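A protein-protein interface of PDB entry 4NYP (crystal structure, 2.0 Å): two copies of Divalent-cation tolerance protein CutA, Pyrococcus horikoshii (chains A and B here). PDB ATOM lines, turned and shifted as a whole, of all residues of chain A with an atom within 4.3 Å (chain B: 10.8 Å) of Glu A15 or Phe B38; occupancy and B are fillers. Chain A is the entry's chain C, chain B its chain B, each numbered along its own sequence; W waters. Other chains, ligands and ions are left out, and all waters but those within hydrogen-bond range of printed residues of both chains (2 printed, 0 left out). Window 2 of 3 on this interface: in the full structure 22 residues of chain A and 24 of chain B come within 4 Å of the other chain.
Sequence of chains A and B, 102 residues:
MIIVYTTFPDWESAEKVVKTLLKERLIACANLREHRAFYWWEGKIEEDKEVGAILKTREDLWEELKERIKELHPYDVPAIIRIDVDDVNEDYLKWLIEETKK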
ATOM      1  N   TRP A  11      -4.233  -9.593  -1.619  1.00  0.00           N
ATOM      2  CA  TRP A  11      -3.125  -8.951  -2.312  1.00  0.00           C
ATOM      3  C   TRP A  11      -2.512  -7.806  -1.531  1.00  0.00           C
ATOM      4  O   TRP A  11      -1.295  -7.611  -1.567  1.00  0.00           O
ATOM      5  CB  TRP A  11      -3.555  -8.439  -3.693  1.00  0.00           C
ATOM      6  CG  TRP A  11      -3.662  -9.511  -4.731  1.00  0.00           C
ATOM      7  CD1 TRP A  11      -4.797 -10.139  -5.149  1.00  0.00           C
ATOM      8  CD2 TRP A  11      -2.586 -10.073  -5.491  1.00  0.00           C
ATOM      9  NE1 TRP A  11      -4.495 -11.059  -6.126  1.00  0.00           N
ATOM     10  CE2 TRP A  11      -3.146 -11.038  -6.357  1.00  0.00           C
ATOM     11  CE3 TRP A  11      -1.202  -9.852  -5.527  1.00  0.00           C
ATOM     12  CZ2 TRP A  11      -2.370 -11.786  -7.252  1.00  0.00           C
ATOM     13  CZ3 TRP A  11      -0.427 -10.595  -6.418  1.00  0.00           C
ATOM     14  CH2 TRP A  11      -1.016 -11.550  -7.268  1.00  0.00           C
ATOM     15  N   GLU A  12      -3.345  -7.037  -0.835  1.00  0.00           N
ATOM     16  CA  GLU A  12      -2.832  -5.918  -0.051  1.00  0.00           C
ATOM     17  C   GLU A  12      -1.709  -6.379   0.893  1.00  0.00           C
ATOM     18  O   GLU A  12      -0.577  -5.887   0.820  1.00  0.00           O
ATOM     19  CB  GLU A  12      -3.962  -5.270   0.754  1.00  0.00           C
ATOM     20  CG  GLU A  12      -3.537  -4.015   1.520  1.00  0.00           C
ATOM     21  CD  GLU A  12      -4.692  -3.354   2.255  1.00  0.00           C
ATOM     22  OE1 GLU A  12      -5.608  -2.824   1.598  1.00  0.00           O
ATOM     23  OE2 GLU A  12      -4.696  -3.372   3.494  1.00  0.00           O
ATOM     24  N   SER A  13      -2.020  -7.330   1.771  1.00  0.00           N
ATOM     25  CA  SER A  13      -1.033  -7.836   2.717  1.00  0.00           C
ATOM     26  C   SER A  13       0.142  -8.514   2.008  1.00  0.00           C
ATOM     27  O   SER A  13       1.302  -8.299   2.364  1.00  0.00           O
ATOM     28  CB  SER A  13      -1.689  -8.820   3.692  1.00  0.00           C
ATOM     29  OG  SER A  13      -2.147  -9.981   3.024  1.00  0.00           O
ATOM     30  N   ALA A  14      -0.158  -9.319   0.996  1.00  0.00           N
ATOM     31  CA  ALA A  14       0.881 -10.028   0.255  1.00  0.00           C
ATOM     32  C   ALA A  14       1.933  -9.072  -0.316  1.00  0.00           C
ATOM     33  O   ALA A  14       3.128  -9.270  -0.110  1.00  0.00           O
ATOM     34  CB  ALA A  14       0.254 -10.848  -0.868  1.00  0.00           C
ATOM     35  N   GLU A  15       1.493  -8.034  -1.027  1.00  0.00           N
ATOM     36  CA  GLU A  15       2.440  -7.076  -1.602  1.00  0.00           C
ATOM     37  C   GLU A  15       3.129  -6.240  -0.525  1.00  0.00           C
ATOM     38  O   GLU A  15       4.322  -5.947  -0.625  1.00  0.00           O
ATOM     39  CB  GLU A  15       1.743  -6.151  -2.607  1.00  0.00           C
ATOM     40  CG  GLU A  15       1.241  -6.862  -3.854  1.00  0.00           C
ATOM     41  CD  GLU A  15       0.899  -5.904  -4.984  1.00  0.00           C
ATOM     42  OE1 GLU A  15       1.127  -4.680  -4.831  1.00  0.00           O
ATOM     43  OE2 GLU A  15       0.409  -6.381  -6.030  1.00  0.00           O
ATOM     44  N   LYS A  16       2.377  -5.863   0.505  1.00  0.00           N
ATOM     45  CA  LYS A  16       2.924  -5.068   1.599  1.00  0.00           C
ATOM     46  C   LYS A  16       4.071  -5.804   2.283  1.00  0.00           C
ATOM     47  O   LYS A  16       5.127  -5.226   2.546  1.00  0.00           O
ATOM     48  CB  LYS A  16       1.840  -4.764   2.634  1.00  0.00           C
ATOM     49  CG  LYS A  16       2.330  -3.980   3.842  1.00  0.00           C
ATOM     50  CD  LYS A  16       1.374  -4.140   5.022  1.00  0.00           C
ATOM     51  CE  LYS A  16       1.239  -5.617   5.416  1.00  0.00           C
ATOM     52  NZ  LYS A  16       0.315  -5.856   6.563  1.00  0.00           N
ATOM     53  N   VAL A  17       3.860  -7.085   2.570  1.00  0.00           N
ATOM     54  CA  VAL A  17       4.879  -7.879   3.227  1.00  0.00           C
ATOM     55  C   VAL A  17       6.070  -8.123   2.300  1.00  0.00           C
ATOM     56  O   VAL A  17       7.217  -7.917   2.691  1.00  0.00           O
ATOM     57  CB  VAL A  17       4.302  -9.227   3.714  1.00  0.00           C
ATOM     58  CG1 VAL A  17       5.406 -10.086   4.301  1.00  0.00           C
ATOM     59  CG2 VAL A  17       3.226  -8.980   4.770  1.00  0.00           C
ATOM     60  N   VAL A  18       5.801  -8.544   1.069  1.00  0.00           N
ATOM     61  CA  VAL A  18       6.878  -8.805   0.123  1.00  0.00           C
ATOM     62  C   VAL A  18       7.719  -7.564  -0.188  1.00  0.00           C
ATOM     63  O   VAL A  18       8.940  -7.648  -0.274  1.00  0.00           O
ATOM     64  CB  VAL A  18       6.332  -9.408  -1.190  1.00  0.00           C
ATOM     65  CG1 VAL A  18       7.399  -9.364  -2.268  1.00  0.00           C
ATOM     66  CG2 VAL A  18       5.905 -10.854  -0.948  1.00  0.00           C
ATOM     67  N   LYS A  19       7.078  -6.413  -0.345  1.00  0.00           N
ATOM     68  CA  LYS A  19       7.822  -5.192  -0.639  1.00  0.00           C
ATOM     69  C   LYS A  19       8.684  -4.797   0.551  1.00  0.00           C
ATOM     70  O   LYS A  19       9.750  -4.216   0.378  1.00  0.00           O
ATOM     71  CB  LYS A  19       6.865  -4.056  -1.014  1.00  0.00           C
ATOM     72  CG  LYS A  19       6.193  -4.272  -2.369  1.00  0.00           C
ATOM     73  CD  LYS A  19       5.205  -3.163  -2.711  1.00  0.00           C
ATOM     74  CE  LYS A  19       4.537  -3.418  -4.061  1.00  0.00           C
ATOM     75  NZ  LYS A  19       3.522  -2.376  -4.401  1.00  0.00           N
ATOM     76  N   LEU A  22      11.662  -7.049   0.529  1.00  0.00           N
ATOM     77  CA  LEU A  22      12.535  -6.586  -0.545  1.00  0.00           C
ATOM     78  C   LEU A  22      13.300  -5.338  -0.092  1.00  0.00           C
ATOM     79  O   LEU A  22      14.518  -5.247  -0.260  1.00  0.00           O
ATOM     80  CB  LEU A  22      11.707  -6.275  -1.797  1.00  0.00           C
ATOM     81  CG  LEU A  22      11.196  -7.474  -2.608  1.00  0.00           C
ATOM     82  CD1 LEU A  22      10.126  -7.024  -3.588  1.00  0.00           C
ATOM     83  CD2 LEU A  22      12.365  -8.119  -3.353  1.00  0.00           C
ATOM     84  N   CSD A  29      13.792 -11.513  -4.730  1.00  0.00           N
ATOM     85  CA  CSD A  29      12.620 -11.516  -5.591  1.00  0.00           C
ATOM     86  CB  CSD A  29      13.054 -11.992  -6.976  1.00  0.00           C
ATOM     87  SG  CSD A  29      11.826 -12.881  -7.930  1.00  0.00           S
ATOM     88  C   CSD A  29      11.469 -12.379  -5.076  1.00  0.00           C
ATOM     89  O   CSD A  29      11.677 -13.307  -4.292  1.00  0.00           O
ATOM     90  OD1 CSD A  29      11.068 -11.891  -8.689  1.00  0.00           O
ATOM     91  OD2 CSD A  29      12.537 -13.852  -8.757  1.00  0.00           O
ATOM     92  N   ALA A  30      10.257 -12.058  -5.527  1.00  0.00           N
ATOM     93  CA  ALA A  30       9.057 -12.803  -5.154  1.00  0.00           C
ATOM     94  C   ALA A  30       8.107 -12.956  -6.346  1.00  0.00           C
ATOM     95  O   ALA A  30       8.013 -12.071  -7.200  1.00  0.00           O
ATOM     96  CB  ALA A  30       8.331 -12.095  -4.011  1.00  0.00           C
ATOM     97  N   LEU A  32       4.105 -13.781  -7.040  1.00  0.00           N
ATOM     98  CA  LEU A  32       2.789 -13.882  -6.404  1.00  0.00           C
ATOM     99  C   LEU A  32       1.682 -14.285  -7.381  1.00  0.00           C
ATOM    100  O   LEU A  32       1.565 -13.717  -8.469  1.00  0.00           O
ATOM    101  CB  LEU A  32       2.409 -12.541  -5.760  1.00  0.00           C
ATOM    102  CG  LEU A  32       2.985 -12.137  -4.402  1.00  0.00           C
ATOM    103  CD1 LEU A  32       4.500 -12.262  -4.392  1.00  0.00           C
ATOM    104  CD2 LEU A  32       2.549 -10.708  -4.099  1.00  0.00           C
ATOM    105  N   TYR B   5      12.303 -24.604 -12.603  1.00  0.00           N
ATOM    106  CA  TYR B   5      11.432 -23.441 -12.596  1.00  0.00           C
ATOM    107  C   TYR B   5      12.107 -22.253 -13.269  1.00  0.00           C
ATOM    108  O   TYR B   5      13.250 -21.919 -12.958  1.00  0.00           O
ATOM    109  CB  TYR B   5      11.066 -23.075 -11.156  1.00  0.00           C
ATOM    110  CG  TYR B   5      10.113 -21.903 -11.015  1.00  0.00           C
ATOM    111  CD1 TYR B   5      10.467 -20.781 -10.264  1.00  0.00           C
ATOM    112  CD2 TYR B   5       8.843 -21.931 -11.598  1.00  0.00           C
ATOM    113  CE1 TYR B   5       9.580 -19.717 -10.094  1.00  0.00           C
ATOM    114  CE2 TYR B   5       7.946 -20.874 -11.433  1.00  0.00           C
ATOM    115  CZ  TYR B   5       8.322 -19.772 -10.678  1.00  0.00           C
ATOM    116  OH  TYR B   5       7.436 -18.733 -10.488  1.00  0.00           O
ATOM    117  N   THR B   7      10.974 -18.279 -15.476  1.00  0.00           N
ATOM    118  CA  THR B   7       9.886 -17.335 -15.714  1.00  0.00           C
ATOM    119  C   THR B   7      10.092 -16.628 -17.045  1.00  0.00           C
ATOM    120  O   THR B   7      11.217 -16.507 -17.514  1.00  0.00           O
ATOM    121  CB  THR B   7       9.791 -16.283 -14.583  1.00  0.00           C
ATOM    122  OG1 THR B   7      10.870 -15.348 -14.694  1.00  0.00           O
ATOM    123  CG2 THR B   7       9.870 -16.962 -13.225  1.00  0.00           C
ATOM    124  N   GLU B  34       0.474 -17.808 -14.830  1.00  0.00           N
ATOM    125  CA  GLU B  34       0.869 -16.433 -14.540  1.00  0.00           C
ATOM    126  C   GLU B  34       1.154 -16.111 -13.076  1.00  0.00           C
ATOM    127  O   GLU B  34       0.725 -16.813 -12.163  1.00  0.00           O
ATOM    128  CB  GLU B  34      -0.224 -15.473 -15.015  1.00  0.00           C
ATOM    129  CG  GLU B  34      -0.396 -15.395 -16.514  1.00  0.00           C
ATOM    130  CD  GLU B  34      -1.490 -14.428 -16.911  1.00  0.00           C
ATOM    131  OE1 GLU B  34      -1.339 -13.765 -17.959  1.00  0.00           O
ATOM    132  OE2 GLU B  34      -2.504 -14.340 -16.174  1.00  0.00           O
ATOM    133  N   HIS B  35       1.901 -15.030 -12.873  1.00  0.00           N
ATOM    134  CA  HIS B  35       2.194 -14.530 -11.543  1.00  0.00           C
ATOM    135  C   HIS B  35       2.704 -13.103 -11.663  1.00  0.00           C
ATOM    136  O   HIS B  35       3.023 -12.640 -12.762  1.00  0.00           O
ATOM    137  CB  HIS B  35       3.204 -15.415 -10.796  1.00  0.00           C
ATOM    138  CG  HIS B  35       4.567 -15.466 -11.414  1.00  0.00           C
ATOM    139  ND1 HIS B  35       5.382 -14.360 -11.522  1.00  0.00           N
ATOM    140  CD2 HIS B  35       5.279 -16.508 -11.900  1.00  0.00           C
ATOM    141  CE1 HIS B  35       6.540 -14.719 -12.046  1.00  0.00           C
ATOM    142  NE2 HIS B  35       6.503 -16.017 -12.284  1.00  0.00           N
ATOM    143  N   ARG B  36       2.749 -12.406 -10.535  1.00  0.00           N
ATOM    144  CA  ARG B  36       3.222 -11.030 -10.510  1.00  0.00           C
ATOM    145  C   ARG B  36       4.565 -11.034  -9.807  1.00  0.00           C
ATOM    146  O   ARG B  36       4.689 -11.512  -8.677  1.00  0.00           O
ATOM    147  CB  ARG B  36       2.225 -10.146  -9.763  1.00  0.00           C
ATOM    148  CG  ARG B  36       2.197  -8.715 -10.266  1.00  0.00           C
ATOM    149  CD  ARG B  36       0.926  -7.992  -9.833  1.00  0.00           C
ATOM    150  NE  ARG B  36       0.634  -6.879 -10.731  1.00  0.00           N
ATOM    151  CZ  ARG B  36      -0.141  -6.964 -11.805  1.00  0.00           C
ATOM    152  NH1 ARG B  36      -0.726  -8.108 -12.120  1.00  0.00           N
ATOM    153  NH2 ARG B  36      -0.306  -5.909 -12.583  1.00  0.00           N
ATOM    154  N   ALA B  37       5.574 -10.500 -10.487  1.00  0.00           N
ATOM    155  CA  ALA B  37       6.922 -10.478  -9.951  1.00  0.00           C
ATOM    156  C   ALA B  37       7.370  -9.140  -9.359  1.00  0.00           C
ATOM    157  O   ALA B  37       7.071  -8.072  -9.901  1.00  0.00           O
ATOM    158  CB  ALA B  37       7.892 -10.912 -11.039  1.00  0.00           C
ATOM    159  N   PHE B  38       8.083  -9.225  -8.238  1.00  0.00           N
ATOM    160  CA  PHE B  38       8.646  -8.064  -7.546  1.00  0.00           C
ATOM    161  C   PHE B  38      10.108  -8.425  -7.289  1.00  0.00           C
ATOM    162  O   PHE B  38      10.405  -9.426  -6.634  1.00  0.00           O
ATOM    163  CB  PHE B  38       7.916  -7.797  -6.221  1.00  0.00           C
ATOM    164  CG  PHE B  38       6.442  -7.501  -6.386  1.00  0.00           C
ATOM    165  CD1 PHE B  38       5.523  -8.533  -6.553  1.00  0.00           C
ATOM    166  CD2 PHE B  38       5.982  -6.185  -6.401  1.00  0.00           C
ATOM    167  CE1 PHE B  38       4.168  -8.261  -6.732  1.00  0.00           C
ATOM    168  CE2 PHE B  38       4.624  -5.899  -6.580  1.00  0.00           C
ATOM    169  CZ  PHE B  38       3.715  -6.939  -6.746  1.00  0.00           C
ATOM    170  N   TYR B  39      11.024  -7.616  -7.809  1.00  0.00           N
ATOM    171  CA  TYR B  39      12.441  -7.909  -7.665  1.00  0.00           C
ATOM    172  C   TYR B  39      13.337  -6.684  -7.721  1.00  0.00           C
ATOM    173  O   TYR B  39      12.935  -5.618  -8.186  1.00  0.00           O
ATOM    174  CB  TYR B  39      12.876  -8.865  -8.776  1.00  0.00           C
ATOM    175  CG  TYR B  39      12.576  -8.331 -10.161  1.00  0.00           C
ATOM    176  CD1 TYR B  39      11.273  -8.329 -10.661  1.00  0.00           C
ATOM    177  CD2 TYR B  39      13.587  -7.789 -10.956  1.00  0.00           C
ATOM    178  CE1 TYR B  39      10.981  -7.801 -11.916  1.00  0.00           C
ATOM    179  CE2 TYR B  39      13.309  -7.256 -12.213  1.00  0.00           C
ATOM    180  CZ  TYR B  39      12.004  -7.263 -12.687  1.00  0.00           C
ATOM    181  OH  TYR B  39      11.718  -6.721 -13.920  1.00  0.00           O
ATOM    182  N   TRP B  40      14.570  -6.867  -7.258  1.00  0.00           N
ATOM    183  CA  TRP B  40      15.567  -5.811  -7.266  1.00  0.00           C
ATOM    184  C   TRP B  40      16.263  -5.774  -8.610  1.00  0.00           C
ATOM    185  O   TRP B  40      16.643  -6.816  -9.155  1.00  0.00           O
ATOM    186  CB  TRP B  40      16.626  -6.051  -6.192  1.00  0.00           C
ATOM    187  CG  TRP B  40      16.267  -5.534  -4.860  1.00  0.00           C
ATOM    188  CD1 TRP B  40      15.893  -6.261  -3.772  1.00  0.00           C
ATOM    189  CD2 TRP B  40      16.241  -4.160  -4.459  1.00  0.00           C
ATOM    190  NE1 TRP B  40      15.633  -5.428  -2.715  1.00  0.00           N
ATOM    191  CE2 TRP B  40      15.838  -4.131  -3.106  1.00  0.00           C
ATOM    192  CE3 TRP B  40      16.521  -2.952  -5.112  1.00  0.00           C
ATOM    193  CZ2 TRP B  40      15.703  -2.936  -2.384  1.00  0.00           C
ATOM    194  CZ3 TRP B  40      16.388  -1.759  -4.396  1.00  0.00           C
ATOM    195  CH2 TRP B  40      15.982  -1.763  -3.046  1.00  0.00           C
ATOM    196  N   TRP B  41      16.422  -4.574  -9.151  1.00  0.00           N
ATOM    197  CA  TRP B  41      17.115  -4.405 -10.415  1.00  0.00           C
ATOM    198  C   TRP B  41      17.819  -3.062 -10.412  1.00  0.00           C
ATOM    199  O   TRP B  41      17.199  -2.015 -10.607  1.00  0.00           O
ATOM    200  CB  TRP B  41      16.151  -4.494 -11.603  1.00  0.00           C
ATOM    201  CG  TRP B  41      16.884  -4.678 -12.903  1.00  0.00           C
ATOM    202  CD1 TRP B  41      17.046  -3.752 -13.898  1.00  0.00           C
ATOM    203  CD2 TRP B  41      17.635  -5.833 -13.306  1.00  0.00           C
ATOM    204  NE1 TRP B  41      17.853  -4.258 -14.890  1.00  0.00           N
ATOM    205  CE2 TRP B  41      18.229  -5.532 -14.552  1.00  0.00           C
ATOM    206  CE3 TRP B  41      17.865  -7.092 -12.732  1.00  0.00           C
ATOM    207  CZ2 TRP B  41      19.044  -6.446 -15.235  1.00  0.00           C
ATOM    208  CZ3 TRP B  41      18.678  -8.002 -13.413  1.00  0.00           C
ATOM    209  CH2 TRP B  41      19.255  -7.672 -14.651  1.00  0.00           C
ATOM    210  N   LYS B  44      16.570  -0.405  -7.723  1.00  0.00           N
ATOM    211  CA  LYS B  44      15.123  -0.186  -7.699  1.00  0.00           C
ATOM    212  C   LYS B  44      14.291  -1.470  -7.662  1.00  0.00           C
ATOM    213  O   LYS B  44      14.657  -2.481  -8.254  1.00  0.00           O
ATOM    214  CB  LYS B  44      14.714   0.653  -8.911  1.00  0.00           C
ATOM    215  CG  LYS B  44      15.292   0.130 -10.207  1.00  0.00           C
ATOM    216  CD  LYS B  44      15.053   1.068 -11.373  1.00  0.00           C
ATOM    217  CE  LYS B  44      15.836   0.595 -12.592  1.00  0.00           C
ATOM    218  NZ  LYS B  44      15.582  -0.850 -12.880  1.00  0.00           N
ATOM    219  N   ILE B  45      13.170  -1.419  -6.952  1.00  0.00           N
ATOM    220  CA  ILE B  45      12.280  -2.568  -6.849  1.00  0.00           C
ATOM    221  C   ILE B  45      11.304  -2.536  -8.023  1.00  0.00           C
ATOM    222  O   ILE B  45      10.390  -1.714  -8.057  1.00  0.00           O
ATOM    223  CB  ILE B  45      11.494  -2.538  -5.520  1.00  0.00           C
ATOM    224  CG1 ILE B  45      12.469  -2.660  -4.344  1.00  0.00           C
ATOM    225  CG2 ILE B  45      10.473  -3.677  -5.483  1.00  0.00           C
ATOM    226  CD1 ILE B  45      11.818  -2.519  -2.989  1.00  0.00           C
ATOM    227  N   GLU B  46      11.509  -3.432  -8.985  1.00  0.00           N
ATOM    228  CA  GLU B  46      10.660  -3.510 -10.173  1.00  0.00           C
ATOM    229  C   GLU B  46       9.438  -4.401  -9.953  1.00  0.00           C
ATOM    230  O   GLU B  46       9.434  -5.266  -9.072  1.00  0.00           O
ATOM    231  CB  GLU B  46      11.454  -4.071 -11.358  1.00  0.00           C
ATOM    232  CG  GLU B  46      12.646  -3.238 -11.815  1.00  0.00           C
ATOM    233  CD  GLU B  46      12.242  -1.920 -12.442  1.00  0.00           C
ATOM    234  OE1 GLU B  46      11.394  -1.927 -13.360  1.00  0.00           O
ATOM    235  OE2 GLU B  46      12.781  -0.874 -12.022  1.00  0.00           O
ATOM    236  N   GLU B  47       8.411  -4.183 -10.770  1.00  0.00           N
ATOM    237  CA  GLU B  47       7.184  -4.965 -10.715  1.00  0.00           C
ATOM    238  C   GLU B  47       6.825  -5.372 -12.144  1.00  0.00           C
ATOM    239  O   GLU B  47       6.716  -4.516 -13.021  1.00  0.00           O
ATOM    240  CB  GLU B  47       6.048  -4.132 -10.121  1.00  0.00           C
ATOM    241  CG  GLU B  47       4.775  -4.919  -9.885  1.00  0.00           C
ATOM    242  CD  GLU B  47       3.610  -4.038  -9.489  1.00  0.00           C
ATOM    243  OE1 GLU B  47       3.761  -3.237  -8.542  1.00  0.00           O
ATOM    244  OE2 GLU B  47       2.542  -4.156 -10.126  1.00  0.00           O
ATOM    245  N   ASP B  48       6.636  -6.668 -12.380  1.00  0.00           N
ATOM    246  CA  ASP B  48       6.305  -7.145 -13.721  1.00  0.00           C
ATOM    247  C   ASP B  48       5.475  -8.415 -13.732  1.00  0.00           C
ATOM    248  O   ASP B  48       5.670  -9.311 -12.907  1.00  0.00           O
ATOM    249  CB  ASP B  48       7.582  -7.417 -14.528  1.00  0.00           C
ATOM    250  CG  ASP B  48       8.180  -6.163 -15.127  1.00  0.00           C
ATOM    251  OD1 ASP B  48       7.565  -5.584 -16.045  1.00  0.00           O
ATOM    252  OD2 ASP B  48       9.270  -5.759 -14.680  1.00  0.00           O
ATOM    253  N   LYS B  49       4.550  -8.489 -14.682  1.00  0.00           N
ATOM    254  CA  LYS B  49       3.726  -9.670 -14.841  1.00  0.00           C
ATOM    255  C   LYS B  49       4.617 -10.669 -15.568  1.00  0.00           C
ATOM    256  O   LYS B  49       5.435 -10.278 -16.402  1.00  0.00           O
ATOM    257  CB  LYS B  49       2.493  -9.377 -15.704  1.00  0.00           C
ATOM    258  CG  LYS B  49       1.447  -8.472 -15.059  1.00  0.00           C
ATOM    259  CD  LYS B  49       0.111  -8.528 -15.808  1.00  0.00           C
ATOM    260  CE  LYS B  49       0.257  -8.203 -17.292  1.00  0.00           C
ATOM    261  NZ  LYS B  49       0.864  -6.863 -17.525  1.00  0.00           N
ATOM    262  N   GLU B  50       4.458 -11.949 -15.252  1.00  0.00           N
ATOM    263  CA  GLU B  50       5.251 -12.990 -15.894  1.00  0.00           C
ATOM    264  C   GLU B  50       4.457 -14.275 -16.041  1.00  0.00           C
ATOM    265  O   GLU B  50       3.376 -14.426 -15.480  1.00  0.00           O
ATOM    266  CB  GLU B  50       6.501 -13.321 -15.075  1.00  0.00           C
ATOM    267  CG  GLU B  50       7.495 -12.195 -14.898  1.00  0.00           C
ATOM    268  CD  GLU B  50       8.809 -12.685 -14.312  1.00  0.00           C
ATOM    269  OE1 GLU B  50       8.808 -13.171 -13.165  1.00  0.00           O
ATOM    270  OE2 GLU B  50       9.844 -12.595 -15.006  1.00  0.00           O
ATOM    271  N   TYR B  75      15.136 -13.135 -21.471  1.00  0.00           N
ATOM    272  CA  TYR B  75      15.821 -12.391 -20.408  1.00  0.00           C
ATOM    273  C   TYR B  75      17.329 -12.591 -20.513  1.00  0.00           C
ATOM    274  O   TYR B  75      17.784 -13.668 -20.894  1.00  0.00           O
ATOM    275  CB  TYR B  75      15.398 -12.867 -19.013  1.00  0.00           C
ATOM    276  CG  TYR B  75      13.995 -12.505 -18.572  1.00  0.00           C
ATOM    277  CD1 TYR B  75      13.286 -11.461 -19.173  1.00  0.00           C
ATOM    278  CD2 TYR B  75      13.393 -13.187 -17.513  1.00  0.00           C
ATOM    279  CE1 TYR B  75      12.010 -11.106 -18.727  1.00  0.00           C
ATOM    280  CE2 TYR B  75      12.122 -12.841 -17.059  1.00  0.00           C
ATOM    281  CZ  TYR B  75      11.438 -11.803 -17.668  1.00  0.00           C
ATOM    282  OH  TYR B  75      10.190 -11.471 -17.213  1.00  0.00           O
HETATM  283  O   HOH W   1       1.301  -3.426  -7.104  1.00  0.00           O
HETATM  284  O   HOH W   2      10.670 -13.418 -11.412  1.00  0.00           O
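NE1 of Trp B40 is in hydrogen-bond range of O of Leu A22 (2.7 Å). The backbone NH (N) of Ala A30 lies within hydrogen-bond range of the backbone carbonyl oxygen (O) of Phe B38. The backbone NH (N) of Arg B36 sits at hydrogen-bond distance from the backbone carbonyl oxygen (O) of Leu A32 (2.7 Å). OD1 of CSD A29 lies close to the backbone carbonyl oxygen (O) of Phe B38, 3.3 Å away.
NE of Arg B36 lies within salt-bridge range of OE2 of Glu B47 (3.4 Å). The side-chain hydroxyl (OH) of Tyr B5 is in hydrogen-bond range of a ring nitrogen (NE2) of His B35 (3.4 Å). The backbone carbonyl oxygen (O) of His B35 lies within hydrogen-bond range of the backbone NH (N) of Glu B50 (3.0 Å). NZ of Lys A19 lies within salt-bridge range of OE1 of Glu A15. N of Ala B37 sits at hydrogen-bond distance from O of Asp B48 (2.7 Å). OH of Tyr B39 lies within hydrogen-bond range of OD2 of Asp B48.
OE2 of Glu A15 touches CZ of Phe B38, 3.4 Å away. Phe B38 touches Lys A19 (CE2 to CE, 3.5 Å). Leu A22 touches Phe B38 (CD1 to CB, 3.5 Å). Ile B45 touches Leu A22. OD1 of CSD A29 touches CB of Tyr B39 (3.5 Å). O of Ala A30 touches O of Arg B36 (3.7 Å). Ala B37 touches Ala A30. O of Leu A32 touches CA of His B35, at 3.2 Å. CE1 of Phe B38 touches CD2 of Leu A32 (3.9 Å).
Of chain B, only Phe B38 (3.4 Å) comes within 4 Å of Glu A15. Of the printed residues of chain A, Phe B38 touches Glu A15 (3.4 Å), Lys A19 (3.5 Å), Leu A22 (3.5 Å), CSD A29 (3.2 Å), Ala A30 (2.9 Å) and Leu A32 (3.9 Å). No residue of chain B comes within 4 Å of Ala A14. No residue of chain B comes within 4 Å of Val A18. Lys A19 touches one residue of chain B. Of chain B, only Phe B38 and Tyr B39 come within 4 Å of CSD A29. Ala A30 touches just these residues of chain B: Arg B36, Ala B37 and Phe B38. Of chain B, only His B35 (3.2 Å), Arg B36 (2.7 Å) and Phe B38 (3.9 Å) come within 4 Å of Leu A32. Printed residues of chain A within 4 Å of Arg B36: Ala A30 and Leu A32. Printed residues of chain A within 4 Å of Ala B37: Ala A30 (3.4 Å). Of the printed residues of chain A, Trp B40 touches Leu A22 (2.7 Å). Tyr B75 touches none of the printed residues of chain A. The nearest printed residue of chain A that does not touch Phe B38 is Val A18 (4.3 Å). The nearest printed residue of chain A that does not touch Arg B36 is Glu A15 (4.2 Å).
Of the 13 printed residues of chain A, 6 touch a printed residue of chain B. Along chain A the printed residues that touch a printed residue of chain B span positions 15 to 32. Among the printed residues, 13 pairs touch across the chains. Among the printed residues, no Asp or Glu carboxylate lies within 4 Å of a Lys or Arg side-chain nitrogen of the other chain.
No position is printed for both chains.
Water W2 bridges OE1 of Glu B50 (2.6 Å) and OD1 of CSD A29 (3.1 Å). Water W1 bridges the side-chain carboxylate of Glu A15 (2.6 Å) and the side-chain carboxylate of Glu B47 (2.9 Å).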
